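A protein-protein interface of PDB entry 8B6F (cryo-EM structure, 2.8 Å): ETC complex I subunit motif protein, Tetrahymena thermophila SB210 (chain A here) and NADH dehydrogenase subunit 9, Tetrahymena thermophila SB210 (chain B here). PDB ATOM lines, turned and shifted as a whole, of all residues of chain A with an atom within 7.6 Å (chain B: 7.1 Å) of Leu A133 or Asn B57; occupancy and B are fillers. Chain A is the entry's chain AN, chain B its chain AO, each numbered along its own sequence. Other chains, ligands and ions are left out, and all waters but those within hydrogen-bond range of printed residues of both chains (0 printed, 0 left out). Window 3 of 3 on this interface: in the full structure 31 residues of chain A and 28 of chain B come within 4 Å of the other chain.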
ATOM      1  N   LYS A  60      -5.751 -26.305 -13.971  1.00  0.00           N
ATOM      2  CA  LYS A  60      -5.152 -26.141 -15.286  1.00  0.00           C
ATOM      3  C   LYS A  60      -5.235 -27.444 -16.070  1.00  0.00           C
ATOM      4  O   LYS A  60      -5.126 -28.536 -15.507  1.00  0.00           O
ATOM      5  CB  LYS A  60      -3.695 -25.702 -15.164  1.00  0.00           C
ATOM      6  CG  LYS A  60      -3.508 -24.321 -14.561  1.00  0.00           C
ATOM      7  CD  LYS A  60      -2.062 -23.855 -14.662  1.00  0.00           C
ATOM      8  CE  LYS A  60      -1.109 -24.770 -13.909  1.00  0.00           C
ATOM      9  NZ  LYS A  60      -1.480 -24.920 -12.476  1.00  0.00           N
ATOM     10  N   THR A  63       0.380 -28.281 -17.186  1.00  0.00           N
ATOM     11  CA  THR A  63       1.319 -27.442 -16.453  1.00  0.00           C
ATOM     12  C   THR A  63       2.144 -26.542 -17.361  1.00  0.00           C
ATOM     13  O   THR A  63       2.654 -25.518 -16.896  1.00  0.00           O
ATOM     14  CB  THR A  63       2.265 -28.307 -15.617  1.00  0.00           C
ATOM     15  OG1 THR A  63       2.899 -29.277 -16.458  1.00  0.00           O
ATOM     16  CG2 THR A  63       1.509 -29.020 -14.513  1.00  0.00           C
ATOM     17  N   TYR A  65       4.953 -27.566 -18.772  1.00  0.00           N
ATOM     18  CA  TYR A  65       6.279 -28.160 -18.796  1.00  0.00           C
ATOM     19  C   TYR A  65       6.173 -29.632 -19.169  1.00  0.00           C
ATOM     20  O   TYR A  65       5.202 -30.311 -18.822  1.00  0.00           O
ATOM     21  CB  TYR A  65       6.974 -28.026 -17.439  1.00  0.00           C
ATOM     22  CG  TYR A  65       7.237 -26.601 -17.021  1.00  0.00           C
ATOM     23  CD1 TYR A  65       6.271 -25.865 -16.350  1.00  0.00           C
ATOM     24  CD2 TYR A  65       8.454 -25.995 -17.287  1.00  0.00           C
ATOM     25  CE1 TYR A  65       6.509 -24.563 -15.962  1.00  0.00           C
ATOM     26  CE2 TYR A  65       8.702 -24.694 -16.902  1.00  0.00           C
ATOM     27  CZ  TYR A  65       7.725 -23.983 -16.240  1.00  0.00           C
ATOM     28  OH  TYR A  65       7.969 -22.687 -15.856  1.00  0.00           O
ATOM     29  N   LEU A  68       5.615 -32.969 -16.428  1.00  0.00           N
ATOM     30  CA  LEU A  68       5.255 -32.330 -15.162  1.00  0.00           C
ATOM     31  C   LEU A  68       3.736 -32.400 -15.041  1.00  0.00           C
ATOM     32  O   LEU A  68       3.026 -31.502 -15.500  1.00  0.00           O
ATOM     33  CB  LEU A  68       5.770 -30.895 -15.099  1.00  0.00           C
ATOM     34  CG  LEU A  68       5.584 -30.160 -13.769  1.00  0.00           C
ATOM     35  CD1 LEU A  68       6.384 -30.821 -12.662  1.00  0.00           C
ATOM     36  CD2 LEU A  68       5.973 -28.699 -13.904  1.00  0.00           C
ATOM     37  N   ASP A  69       3.241 -33.468 -14.419  1.00  0.00           N
ATOM     38  CA  ASP A  69       1.809 -33.682 -14.304  1.00  0.00           C
ATOM     39  C   ASP A  69       1.179 -32.657 -13.365  1.00  0.00           C
ATOM     40  O   ASP A  69       1.849 -32.030 -12.542  1.00  0.00           O
ATOM     41  CB  ASP A  69       1.514 -35.094 -13.799  1.00  0.00           C
ATOM     42  CG  ASP A  69       1.919 -36.165 -14.791  1.00  0.00           C
ATOM     43  OD1 ASP A  69       2.437 -35.812 -15.872  1.00  0.00           O
ATOM     44  OD2 ASP A  69       1.715 -37.360 -14.494  1.00  0.00           O
ATOM     45  N   ASP A 129       3.758 -18.733 -12.148  1.00  0.00           N
ATOM     46  CA  ASP A 129       4.036 -19.983 -12.833  1.00  0.00           C
ATOM     47  C   ASP A 129       3.132 -21.084 -12.280  1.00  0.00           C
ATOM     48  O   ASP A 129       2.328 -20.869 -11.370  1.00  0.00           O
ATOM     49  CB  ASP A 129       5.515 -20.347 -12.684  1.00  0.00           C
ATOM     50  CG  ASP A 129       6.006 -21.255 -13.793  1.00  0.00           C
ATOM     51  OD1 ASP A 129       5.179 -21.979 -14.382  1.00  0.00           O
ATOM     52  OD2 ASP A 129       7.223 -21.245 -14.077  1.00  0.00           O
ATOM     53  N   SER A 130       3.268 -22.282 -12.844  1.00  0.00           N
ATOM     54  CA  SER A 130       2.462 -23.411 -12.400  1.00  0.00           C
ATOM     55  C   SER A 130       2.745 -23.729 -10.937  1.00  0.00           C
ATOM     56  O   SER A 130       3.883 -23.631 -10.470  1.00  0.00           O
ATOM     57  CB  SER A 130       2.753 -24.638 -13.263  1.00  0.00           C
ATOM     58  OG  SER A 130       2.522 -24.365 -14.633  1.00  0.00           O
ATOM     59  N   ILE A 131       1.692 -24.107 -10.209  1.00  0.00           N
ATOM     60  CA  ILE A 131       1.864 -24.483  -8.811  1.00  0.00           C
ATOM     61  C   ILE A 131       2.707 -25.744  -8.697  1.00  0.00           C
ATOM     62  O   ILE A 131       3.381 -25.960  -7.685  1.00  0.00           O
ATOM     63  CB  ILE A 131       0.491 -24.657  -8.134  1.00  0.00           C
ATOM     64  CG1 ILE A 131       0.633 -24.671  -6.611  1.00  0.00           C
ATOM     65  CG2 ILE A 131      -0.194 -25.935  -8.608  1.00  0.00           C
ATOM     66  CD1 ILE A 131       0.978 -23.323  -6.014  1.00  0.00           C
ATOM     67  N   GLU A 132       2.697 -26.589  -9.730  1.00  0.00           N
ATOM     68  CA  GLU A 132       3.451 -27.836  -9.669  1.00  0.00           C
ATOM     69  C   GLU A 132       4.947 -27.573  -9.597  1.00  0.00           C
ATOM     70  O   GLU A 132       5.670 -28.267  -8.875  1.00  0.00           O
ATOM     71  CB  GLU A 132       3.118 -28.710 -10.877  1.00  0.00           C
ATOM     72  CG  GLU A 132       1.714 -29.300 -10.850  1.00  0.00           C
ATOM     73  CD  GLU A 132       0.628 -28.262 -11.043  1.00  0.00           C
ATOM     74  OE1 GLU A 132       0.948 -27.138 -11.480  1.00  0.00           O
ATOM     75  OE2 GLU A 132      -0.547 -28.572 -10.762  1.00  0.00           O
ATOM     76  N   LEU A 133       5.434 -26.582 -10.344  1.00  0.00           N
ATOM     77  CA  LEU A 133       6.850 -26.240 -10.272  1.00  0.00           C
ATOM     78  C   LEU A 133       7.221 -25.750  -8.880  1.00  0.00           C
ATOM     79  O   LEU A 133       8.283 -26.100  -8.352  1.00  0.00           O
ATOM     80  CB  LEU A 133       7.186 -25.184 -11.324  1.00  0.00           C
ATOM     81  CG  LEU A 133       8.655 -24.776 -11.437  1.00  0.00           C
ATOM     82  CD1 LEU A 133       9.526 -25.966 -11.798  1.00  0.00           C
ATOM     83  CD2 LEU A 133       8.811 -23.668 -12.462  1.00  0.00           C
ATOM     84  N   PHE A 134       6.360 -24.932  -8.270  1.00  0.00           N
ATOM     85  CA  PHE A 134       6.609 -24.477  -6.906  1.00  0.00           C
ATOM     86  C   PHE A 134       6.622 -25.649  -5.933  1.00  0.00           C
ATOM     87  O   PHE A 134       7.451 -25.698  -5.017  1.00  0.00           O
ATOM     88  CB  PHE A 134       5.552 -23.450  -6.498  1.00  0.00           C
ATOM     89  CG  PHE A 134       5.738 -22.909  -5.111  1.00  0.00           C
ATOM     90  CD1 PHE A 134       6.550 -21.811  -4.887  1.00  0.00           C
ATOM     91  CD2 PHE A 134       5.097 -23.494  -4.031  1.00  0.00           C
ATOM     92  CE1 PHE A 134       6.724 -21.307  -3.611  1.00  0.00           C
ATOM     93  CE2 PHE A 134       5.265 -22.996  -2.754  1.00  0.00           C
ATOM     94  CZ  PHE A 134       6.080 -21.901  -2.545  1.00  0.00           C
ATOM     95  N   ILE A 135       5.704 -26.601  -6.110  1.00  0.00           N
ATOM     96  CA  ILE A 135       5.677 -27.784  -5.252  1.00  0.00           C
ATOM     97  C   ILE A 135       6.981 -28.558  -5.383  1.00  0.00           C
ATOM     98  O   ILE A 135       7.580 -28.981  -4.387  1.00  0.00           O
ATOM     99  CB  ILE A 135       4.467 -28.671  -5.601  1.00  0.00           C
ATOM    100  CG1 ILE A 135       3.150 -27.915  -5.391  1.00  0.00           C
ATOM    101  CG2 ILE A 135       4.503 -29.970  -4.795  1.00  0.00           C
ATOM    102  CD1 ILE A 135       2.646 -27.900  -3.982  1.00  0.00           C
ATOM    103  N   TYR A 136       7.440 -28.757  -6.621  1.00  0.00           N
ATOM    104  CA  TYR A 136       8.665 -29.515  -6.841  1.00  0.00           C
ATOM    105  C   TYR A 136       9.866 -28.824  -6.212  1.00  0.00           C
ATOM    106  O   TYR A 136      10.706 -29.473  -5.579  1.00  0.00           O
ATOM    107  CB  TYR A 136       8.881 -29.708  -8.343  1.00  0.00           C
ATOM    108  CG  TYR A 136      10.129 -30.478  -8.691  1.00  0.00           C
ATOM    109  CD1 TYR A 136      10.152 -31.865  -8.645  1.00  0.00           C
ATOM    110  CD2 TYR A 136      11.284 -29.816  -9.082  1.00  0.00           C
ATOM    111  CE1 TYR A 136      11.293 -32.569  -8.968  1.00  0.00           C
ATOM    112  CE2 TYR A 136      12.428 -30.509  -9.406  1.00  0.00           C
ATOM    113  CZ  TYR A 136      12.426 -31.886  -9.348  1.00  0.00           C
ATOM    114  OH  TYR A 136      13.567 -32.579  -9.673  1.00  0.00           O
ATOM    115  N   SER A 137       9.964 -27.504  -6.369  1.00  0.00           N
ATOM    116  CA  SER A 137      11.064 -26.766  -5.762  1.00  0.00           C
ATOM    117  C   SER A 137      10.982 -26.813  -4.241  1.00  0.00           C
ATOM    118  O   SER A 137      12.008 -26.921  -3.562  1.00  0.00           O
ATOM    119  CB  SER A 137      11.063 -25.330  -6.273  1.00  0.00           C
ATOM    120  OG  SER A 137      11.300 -25.327  -7.670  1.00  0.00           O
ATOM    121  N   TYR A 138       9.770 -26.725  -3.693  1.00  0.00           N
ATOM    122  CA  TYR A 138       9.607 -26.721  -2.244  1.00  0.00           C
ATOM    123  C   TYR A 138       9.941 -28.077  -1.640  1.00  0.00           C
ATOM    124  O   TYR A 138      10.415 -28.146  -0.501  1.00  0.00           O
ATOM    125  CB  TYR A 138       8.172 -26.314  -1.900  1.00  0.00           C
ATOM    126  CG  TYR A 138       7.927 -25.976  -0.449  1.00  0.00           C
ATOM    127  CD1 TYR A 138       8.749 -25.093   0.235  1.00  0.00           C
ATOM    128  CD2 TYR A 138       6.841 -26.515   0.225  1.00  0.00           C
ATOM    129  CE1 TYR A 138       8.511 -24.775   1.557  1.00  0.00           C
ATOM    130  CE2 TYR A 138       6.595 -26.205   1.543  1.00  0.00           C
ATOM    131  CZ  TYR A 138       7.431 -25.335   2.205  1.00  0.00           C
ATOM    132  OH  TYR A 138       7.182 -25.027   3.520  1.00  0.00           O
ATOM    133  N   GLY A 139       9.712 -29.160  -2.380  1.00  0.00           N
ATOM    134  CA  GLY A 139       9.998 -30.490  -1.876  1.00  0.00           C
ATOM    135  C   GLY A 139      11.468 -30.779  -1.655  1.00  0.00           C
ATOM    136  O   GLY A 139      11.790 -31.766  -0.985  1.00  0.00           O
ATOM    137  N   LYS A 140      12.363 -29.954  -2.201  1.00  0.00           N
ATOM    138  CA  LYS A 140      13.793 -30.195  -2.062  1.00  0.00           C
ATOM    139  C   LYS A 140      14.330 -29.800  -0.695  1.00  0.00           C
ATOM    140  O   LYS A 140      15.418 -30.247  -0.320  1.00  0.00           O
ATOM    141  CB  LYS A 140      14.562 -29.441  -3.146  1.00  0.00           C
ATOM    142  CG  LYS A 140      14.157 -29.819  -4.557  1.00  0.00           C
ATOM    143  CD  LYS A 140      14.929 -29.019  -5.583  1.00  0.00           C
ATOM    144  CE  LYS A 140      14.430 -29.310  -6.987  1.00  0.00           C
ATOM    145  NZ  LYS A 140      15.153 -28.512  -8.013  1.00  0.00           N
ATOM    146  N   LEU B  49      22.371 -23.550  -2.362  1.00  0.00           N
ATOM    147  CA  LEU B  49      21.768 -22.968  -3.556  1.00  0.00           C
ATOM    148  C   LEU B  49      20.998 -24.012  -4.353  1.00  0.00           C
ATOM    149  O   LEU B  49      19.910 -23.734  -4.868  1.00  0.00           O
ATOM    150  CB  LEU B  49      22.846 -22.332  -4.432  1.00  0.00           C
ATOM    151  CG  LEU B  49      23.497 -21.050  -3.916  1.00  0.00           C
ATOM    152  CD1 LEU B  49      24.687 -20.677  -4.779  1.00  0.00           C
ATOM    153  CD2 LEU B  49      22.486 -19.919  -3.890  1.00  0.00           C
ATOM    154  N   LYS B  50      21.551 -25.219  -4.471  1.00  0.00           N
ATOM    155  CA  LYS B  50      20.968 -26.222  -5.351  1.00  0.00           C
ATOM    156  C   LYS B  50      19.626 -26.744  -4.849  1.00  0.00           C
ATOM    157  O   LYS B  50      18.897 -27.370  -5.625  1.00  0.00           O
ATOM    158  CB  LYS B  50      21.946 -27.387  -5.521  1.00  0.00           C
ATOM    159  CG  LYS B  50      21.492 -28.466  -6.495  1.00  0.00           C
ATOM    160  CD  LYS B  50      21.220 -27.896  -7.876  1.00  0.00           C
ATOM    161  CE  LYS B  50      20.952 -28.998  -8.883  1.00  0.00           C
ATOM    162  NZ  LYS B  50      20.645 -28.442 -10.229  1.00  0.00           N
ATOM    163  N   ARG B  51      19.277 -26.502  -3.582  1.00  0.00           N
ATOM    164  CA  ARG B  51      18.059 -27.083  -3.031  1.00  0.00           C
ATOM    165  C   ARG B  51      17.253 -26.126  -2.161  1.00  0.00           C
ATOM    166  O   ARG B  51      16.257 -26.553  -1.565  1.00  0.00           O
ATOM    167  CB  ARG B  51      18.394 -28.346  -2.232  1.00  0.00           C
ATOM    168  CG  ARG B  51      18.657 -29.543  -3.122  1.00  0.00           C
ATOM    169  CD  ARG B  51      19.075 -30.768  -2.338  1.00  0.00           C
ATOM    170  NE  ARG B  51      19.169 -31.932  -3.211  1.00  0.00           N
ATOM    171  CZ  ARG B  51      20.148 -32.139  -4.082  1.00  0.00           C
ATOM    172  NH1 ARG B  51      21.142 -31.278  -4.223  1.00  0.00           N
ATOM    173  NH2 ARG B  51      20.123 -33.233  -4.837  1.00  0.00           N
ATOM    174  N   GLU B  52      17.636 -24.858  -2.061  1.00  0.00           N
ATOM    175  CA  GLU B  52      16.774 -23.884  -1.410  1.00  0.00           C
ATOM    176  C   GLU B  52      15.569 -23.587  -2.296  1.00  0.00           C
ATOM    177  O   GLU B  52      15.625 -23.721  -3.521  1.00  0.00           O
ATOM    178  CB  GLU B  52      17.549 -22.601  -1.112  1.00  0.00           C
ATOM    179  CG  GLU B  52      16.785 -21.581  -0.286  1.00  0.00           C
ATOM    180  CD  GLU B  52      16.443 -22.091   1.098  1.00  0.00           C
ATOM    181  OE1 GLU B  52      16.933 -23.176   1.474  1.00  0.00           O
ATOM    182  OE2 GLU B  52      15.683 -21.406   1.814  1.00  0.00           O
ATOM    183  N   LEU B  53      14.465 -23.183  -1.664  1.00  0.00           N
ATOM    184  CA  LEU B  53      13.209 -23.024  -2.393  1.00  0.00           C
ATOM    185  C   LEU B  53      13.367 -22.070  -3.572  1.00  0.00           C
ATOM    186  O   LEU B  53      13.213 -22.465  -4.733  1.00  0.00           O
ATOM    187  CB  LEU B  53      12.115 -22.530  -1.446  1.00  0.00           C
ATOM    188  CG  LEU B  53      10.812 -22.065  -2.104  1.00  0.00           C
ATOM    189  CD1 LEU B  53      10.255 -23.123  -3.038  1.00  0.00           C
ATOM    190  CD2 LEU B  53       9.783 -21.698  -1.048  1.00  0.00           C
ATOM    191  N   LEU B  54      13.678 -20.804  -3.290  1.00  0.00           N
ATOM    192  CA  LEU B  54      13.737 -19.812  -4.359  1.00  0.00           C
ATOM    193  C   LEU B  54      14.989 -19.971  -5.209  1.00  0.00           C
ATOM    194  O   LEU B  54      14.991 -19.578  -6.382  1.00  0.00           O
ATOM    195  CB  LEU B  54      13.658 -18.404  -3.774  1.00  0.00           C
ATOM    196  CG  LEU B  54      12.359 -18.071  -3.032  1.00  0.00           C
ATOM    197  CD1 LEU B  54      12.351 -16.616  -2.629  1.00  0.00           C
ATOM    198  CD2 LEU B  54      11.120 -18.392  -3.859  1.00  0.00           C
ATOM    199  N   PHE B  55      16.054 -20.537  -4.651  1.00  0.00           N
ATOM    200  CA  PHE B  55      17.261 -20.818  -5.414  1.00  0.00           C
ATOM    201  C   PHE B  55      17.253 -22.206  -6.034  1.00  0.00           C
ATOM    202  O   PHE B  55      18.240 -22.590  -6.666  1.00  0.00           O
ATOM    203  CB  PHE B  55      18.503 -20.665  -4.532  1.00  0.00           C
ATOM    204  CG  PHE B  55      18.813 -19.247  -4.161  1.00  0.00           C
ATOM    205  CD1 PHE B  55      19.271 -18.354  -5.115  1.00  0.00           C
ATOM    206  CD2 PHE B  55      18.667 -18.811  -2.857  1.00  0.00           C
ATOM    207  CE1 PHE B  55      19.565 -17.049  -4.778  1.00  0.00           C
ATOM    208  CE2 PHE B  55      18.959 -17.507  -2.513  1.00  0.00           C
ATOM    209  CZ  PHE B  55      19.410 -16.624  -3.476  1.00  0.00           C
ATOM    210  N   SER B  56      16.171 -22.968  -5.869  1.00  0.00           N
ATOM    211  CA  SER B  56      16.109 -24.296  -6.469  1.00  0.00           C
ATOM    212  C   SER B  56      16.206 -24.217  -7.986  1.00  0.00           C
ATOM    213  O   SER B  56      16.919 -25.010  -8.612  1.00  0.00           O
ATOM    214  CB  SER B  56      14.819 -25.000  -6.054  1.00  0.00           C
ATOM    215  OG  SER B  56      14.601 -26.154  -6.846  1.00  0.00           O
ATOM    216  N   ASN B  57      15.496 -23.268  -8.596  1.00  0.00           N
ATOM    217  CA  ASN B  57      15.502 -23.101 -10.047  1.00  0.00           C
ATOM    218  C   ASN B  57      16.715 -22.277 -10.486  1.00  0.00           C
ATOM    219  O   ASN B  57      16.602 -21.210 -11.084  1.00  0.00           O
ATOM    220  CB  ASN B  57      14.203 -22.460 -10.511  1.00  0.00           C
ATOM    221  CG  ASN B  57      13.028 -23.404 -10.425  1.00  0.00           C
ATOM    222  OD1 ASN B  57      13.049 -24.369  -9.663  1.00  0.00           O
ATOM    223  ND2 ASN B  57      11.998 -23.142 -11.217  1.00  0.00           N
ATOM    224  N   ILE B  58      17.897 -22.805 -10.176  1.00  0.00           N
ATOM    225  CA  ILE B  58      19.163 -22.135 -10.450  1.00  0.00           C
ATOM    226  C   ILE B  58      20.002 -23.022 -11.359  1.00  0.00           C
ATOM    227  O   ILE B  58      20.090 -24.237 -11.139  1.00  0.00           O
ATOM    228  CB  ILE B  58      19.916 -21.804  -9.149  1.00  0.00           C
ATOM    229  CG1 ILE B  58      21.084 -20.865  -9.445  1.00  0.00           C
ATOM    230  CG2 ILE B  58      20.413 -23.082  -8.475  1.00  0.00           C
ATOM    231  CD1 ILE B  58      21.806 -20.369  -8.209  1.00  0.00           C
ATOM    232  N   THR B  59      20.598 -22.423 -12.386  1.00  0.00           N
ATOM    233  CA  THR B  59      21.470 -23.118 -13.321  1.00  0.00           C
ATOM    234  C   THR B  59      22.820 -22.420 -13.368  1.00  0.00           C
ATOM    235  O   THR B  59      22.890 -21.190 -13.417  1.00  0.00           O
ATOM    236  CB  THR B  59      20.886 -23.162 -14.737  1.00  0.00           C
ATOM    237  OG1 THR B  59      20.981 -21.865 -15.341  1.00  0.00           O
ATOM    238  CG2 THR B  59      19.443 -23.579 -14.704  1.00  0.00           C
ATOM    239  N   TYR B 101      22.175 -18.448 -12.949  1.00  0.00           N
ATOM    240  CA  TYR B 101      20.926 -17.768 -13.262  1.00  0.00           C
ATOM    241  C   TYR B 101      19.788 -18.463 -12.528  1.00  0.00           C
ATOM    242  O   TYR B 101      19.663 -19.690 -12.586  1.00  0.00           O
ATOM    243  CB  TYR B 101      20.657 -17.759 -14.767  1.00  0.00           C
ATOM    244  CG  TYR B 101      19.337 -17.121 -15.125  1.00  0.00           C
ATOM    245  CD1 TYR B 101      19.207 -15.741 -15.180  1.00  0.00           C
ATOM    246  CD2 TYR B 101      18.222 -17.897 -15.404  1.00  0.00           C
ATOM    247  CE1 TYR B 101      18.006 -15.151 -15.503  1.00  0.00           C
ATOM    248  CE2 TYR B 101      17.015 -17.315 -15.727  1.00  0.00           C
ATOM    249  CZ  TYR B 101      16.914 -15.942 -15.775  1.00  0.00           C
ATOM    250  OH  TYR B 101      15.712 -15.358 -16.097  1.00  0.00           O
ATOM    251  N   ASN B 102      18.964 -17.673 -11.847  1.00  0.00           N
ATOM    252  CA  ASN B 102      17.819 -18.161 -11.089  1.00  0.00           C
ATOM    253  C   ASN B 102      16.535 -17.726 -11.779  1.00  0.00           C
ATOM    254  O   ASN B 102      16.363 -16.544 -12.090  1.00  0.00           O
ATOM    255  CB  ASN B 102      17.858 -17.630  -9.654  1.00  0.00           C
ATOM    256  CG  ASN B 102      16.751 -18.196  -8.792  1.00  0.00           C
ATOM    257  OD1 ASN B 102      15.796 -18.785  -9.294  1.00  0.00           O
ATOM    258  ND2 ASN B 102      16.871 -18.014  -7.485  1.00  0.00           N
ATOM    259  N   TYR B 103      15.635 -18.684 -12.010  1.00  0.00           N
ATOM    260  CA  TYR B 103      14.419 -18.407 -12.769  1.00  0.00           C
ATOM    261  C   TYR B 103      13.315 -17.833 -11.892  1.00  0.00           C
ATOM    262  O   TYR B 103      12.571 -16.949 -12.332  1.00  0.00           O
ATOM    263  CB  TYR B 103      13.930 -19.680 -13.459  1.00  0.00           C
ATOM    264  CG  TYR B 103      14.800 -20.121 -14.612  1.00  0.00           C
ATOM    265  CD1 TYR B 103      15.923 -20.907 -14.400  1.00  0.00           C
ATOM    266  CD2 TYR B 103      14.489 -19.760 -15.913  1.00  0.00           C
ATOM    267  CE1 TYR B 103      16.718 -21.313 -15.453  1.00  0.00           C
ATOM    268  CE2 TYR B 103      15.274 -20.161 -16.972  1.00  0.00           C
ATOM    269  CZ  TYR B 103      16.388 -20.937 -16.736  1.00  0.00           C
ATOM    270  OH  TYR B 103      17.172 -21.338 -17.792  1.00  0.00           O
ATOM    271  N   PHE B 104      13.171 -18.328 -10.663  1.00  0.00           N
ATOM    272  CA  PHE B 104      12.131 -17.802  -9.787  1.00  0.00           C
ATOM    273  C   PHE B 104      12.326 -16.315  -9.530  1.00  0.00           C
ATOM    274  O   PHE B 104      11.366 -15.538  -9.580  1.00  0.00           O
ATOM    275  CB  PHE B 104      12.122 -18.556  -8.457  1.00  0.00           C
ATOM    276  CG  PHE B 104      11.387 -19.864  -8.494  1.00  0.00           C
ATOM    277  CD1 PHE B 104      10.219 -20.015  -9.226  1.00  0.00           C
ATOM    278  CD2 PHE B 104      11.859 -20.939  -7.770  1.00  0.00           C
ATOM    279  CE1 PHE B 104       9.550 -21.218  -9.244  1.00  0.00           C
ATOM    280  CE2 PHE B 104      11.197 -22.138  -7.783  1.00  0.00           C
ATOM    281  CZ  PHE B 104      10.038 -22.282  -8.520  1.00  0.00           C
ATOM    282  N   LEU B 105      13.558 -15.898  -9.254  1.00  0.00           N
ATOM    283  CA  LEU B 105      13.858 -14.501  -8.983  1.00  0.00           C
ATOM    284  C   LEU B 105      14.283 -13.730 -10.223  1.00  0.00           C
ATOM    285  O   LEU B 105      14.537 -12.526 -10.124  1.00  0.00           O
ATOM    286  CB  LEU B 105      14.958 -14.405  -7.922  1.00  0.00           C
ATOM    287  CG  LEU B 105      14.691 -15.169  -6.624  1.00  0.00           C
ATOM    288  CD1 LEU B 105      15.872 -15.050  -5.680  1.00  0.00           C
ATOM    289  CD2 LEU B 105      13.423 -14.674  -5.957  1.00  0.00           C
ATOM    290  N   SER B 107      17.056 -13.615 -11.843  1.00  0.00           N
ATOM    291  CA  SER B 107      18.264 -12.944 -11.389  1.00  0.00           C
ATOM    292  C   SER B 107      19.497 -13.682 -11.887  1.00  0.00           C
ATOM    293  O   SER B 107      19.448 -14.864 -12.232  1.00  0.00           O
ATOM    294  CB  SER B 107      18.305 -12.838  -9.859  1.00  0.00           C
ATOM    295  OG  SER B 107      18.363 -14.121  -9.261  1.00  0.00           O
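Among the printed residues, pairs that only touch across the chains: Ser A137 with Phe B104, Leu A133 with Asn B57, Ser A137 with Ser B56, Tyr A138 with Leu B53, Lys A140 with Arg B51, Ser A137 with Leu B53 and Phe A134 with Leu B53.
The backbone carbonyl oxygen (O) of Asn B57 sits close to the side-chain amide oxygen (OD1) of Asn B102 (3.1 Å). O of Leu A133 is in hydrogen-bond range of OG of Ser A137 (3.2 Å). O of Asn B57 lies within hydrogen-bond range of N of Tyr B103 (2.9 Å). The backbone NH (N) of Phe B104 lies within hydrogen-bond range of the side-chain amide oxygen (OD1) of Asn B102 (3.0 Å).
The side-chain amino group (NZ) of Lys A140 sits at hydrogen-bond distance from the side-chain hydroxyl (OG) of Ser B56 (2.7 Å). The side-chain amide oxygen (OD1) of Asn B57 is in hydrogen-bond range of the side-chain hydroxyl (OG) of Ser A137, 2.8 Å away.
Glu A132 touches none of the printed residues of chain B. Of the printed residues of chain B, Ser A137 touches Leu B53, Ser B56, Asn B57 and Phe B104. Of the printed residues of chain B, Lys A140 touches Arg B51 and Ser B56. Ser B56 touches just these residues of chain A: Ser A137 (3.5 Å) and Lys A140 (2.7 Å). Of chain A, only Leu A133 and Ser A137 come within 4 Å of Asn B57. Tyr B101 touches none of the printed residues of chain A. The nearest residue of chain B that does not touch Leu A133 is Phe B104 (4.1 Å). The nearest printed residue of chain A that does not touch Phe B104 is Leu A133 (4.1 Å).
Of the 17 printed residues of chain B, 5 touch a printed residue of chain A. Printed residues of chain B that touch a printed residue of chain A: Arg B51, Leu B53, Ser B56, Asn B57 and Phe B104. Hydrophobic or aromatic side chains of chain A within 4 Å of the printed part of chain B: Leu A133, Phe A134 and Tyr A138. Among the printed residues, no Asp or Glu carboxylate lies within 4 Å of a Lys or Arg side-chain nitrogen of the other chain.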
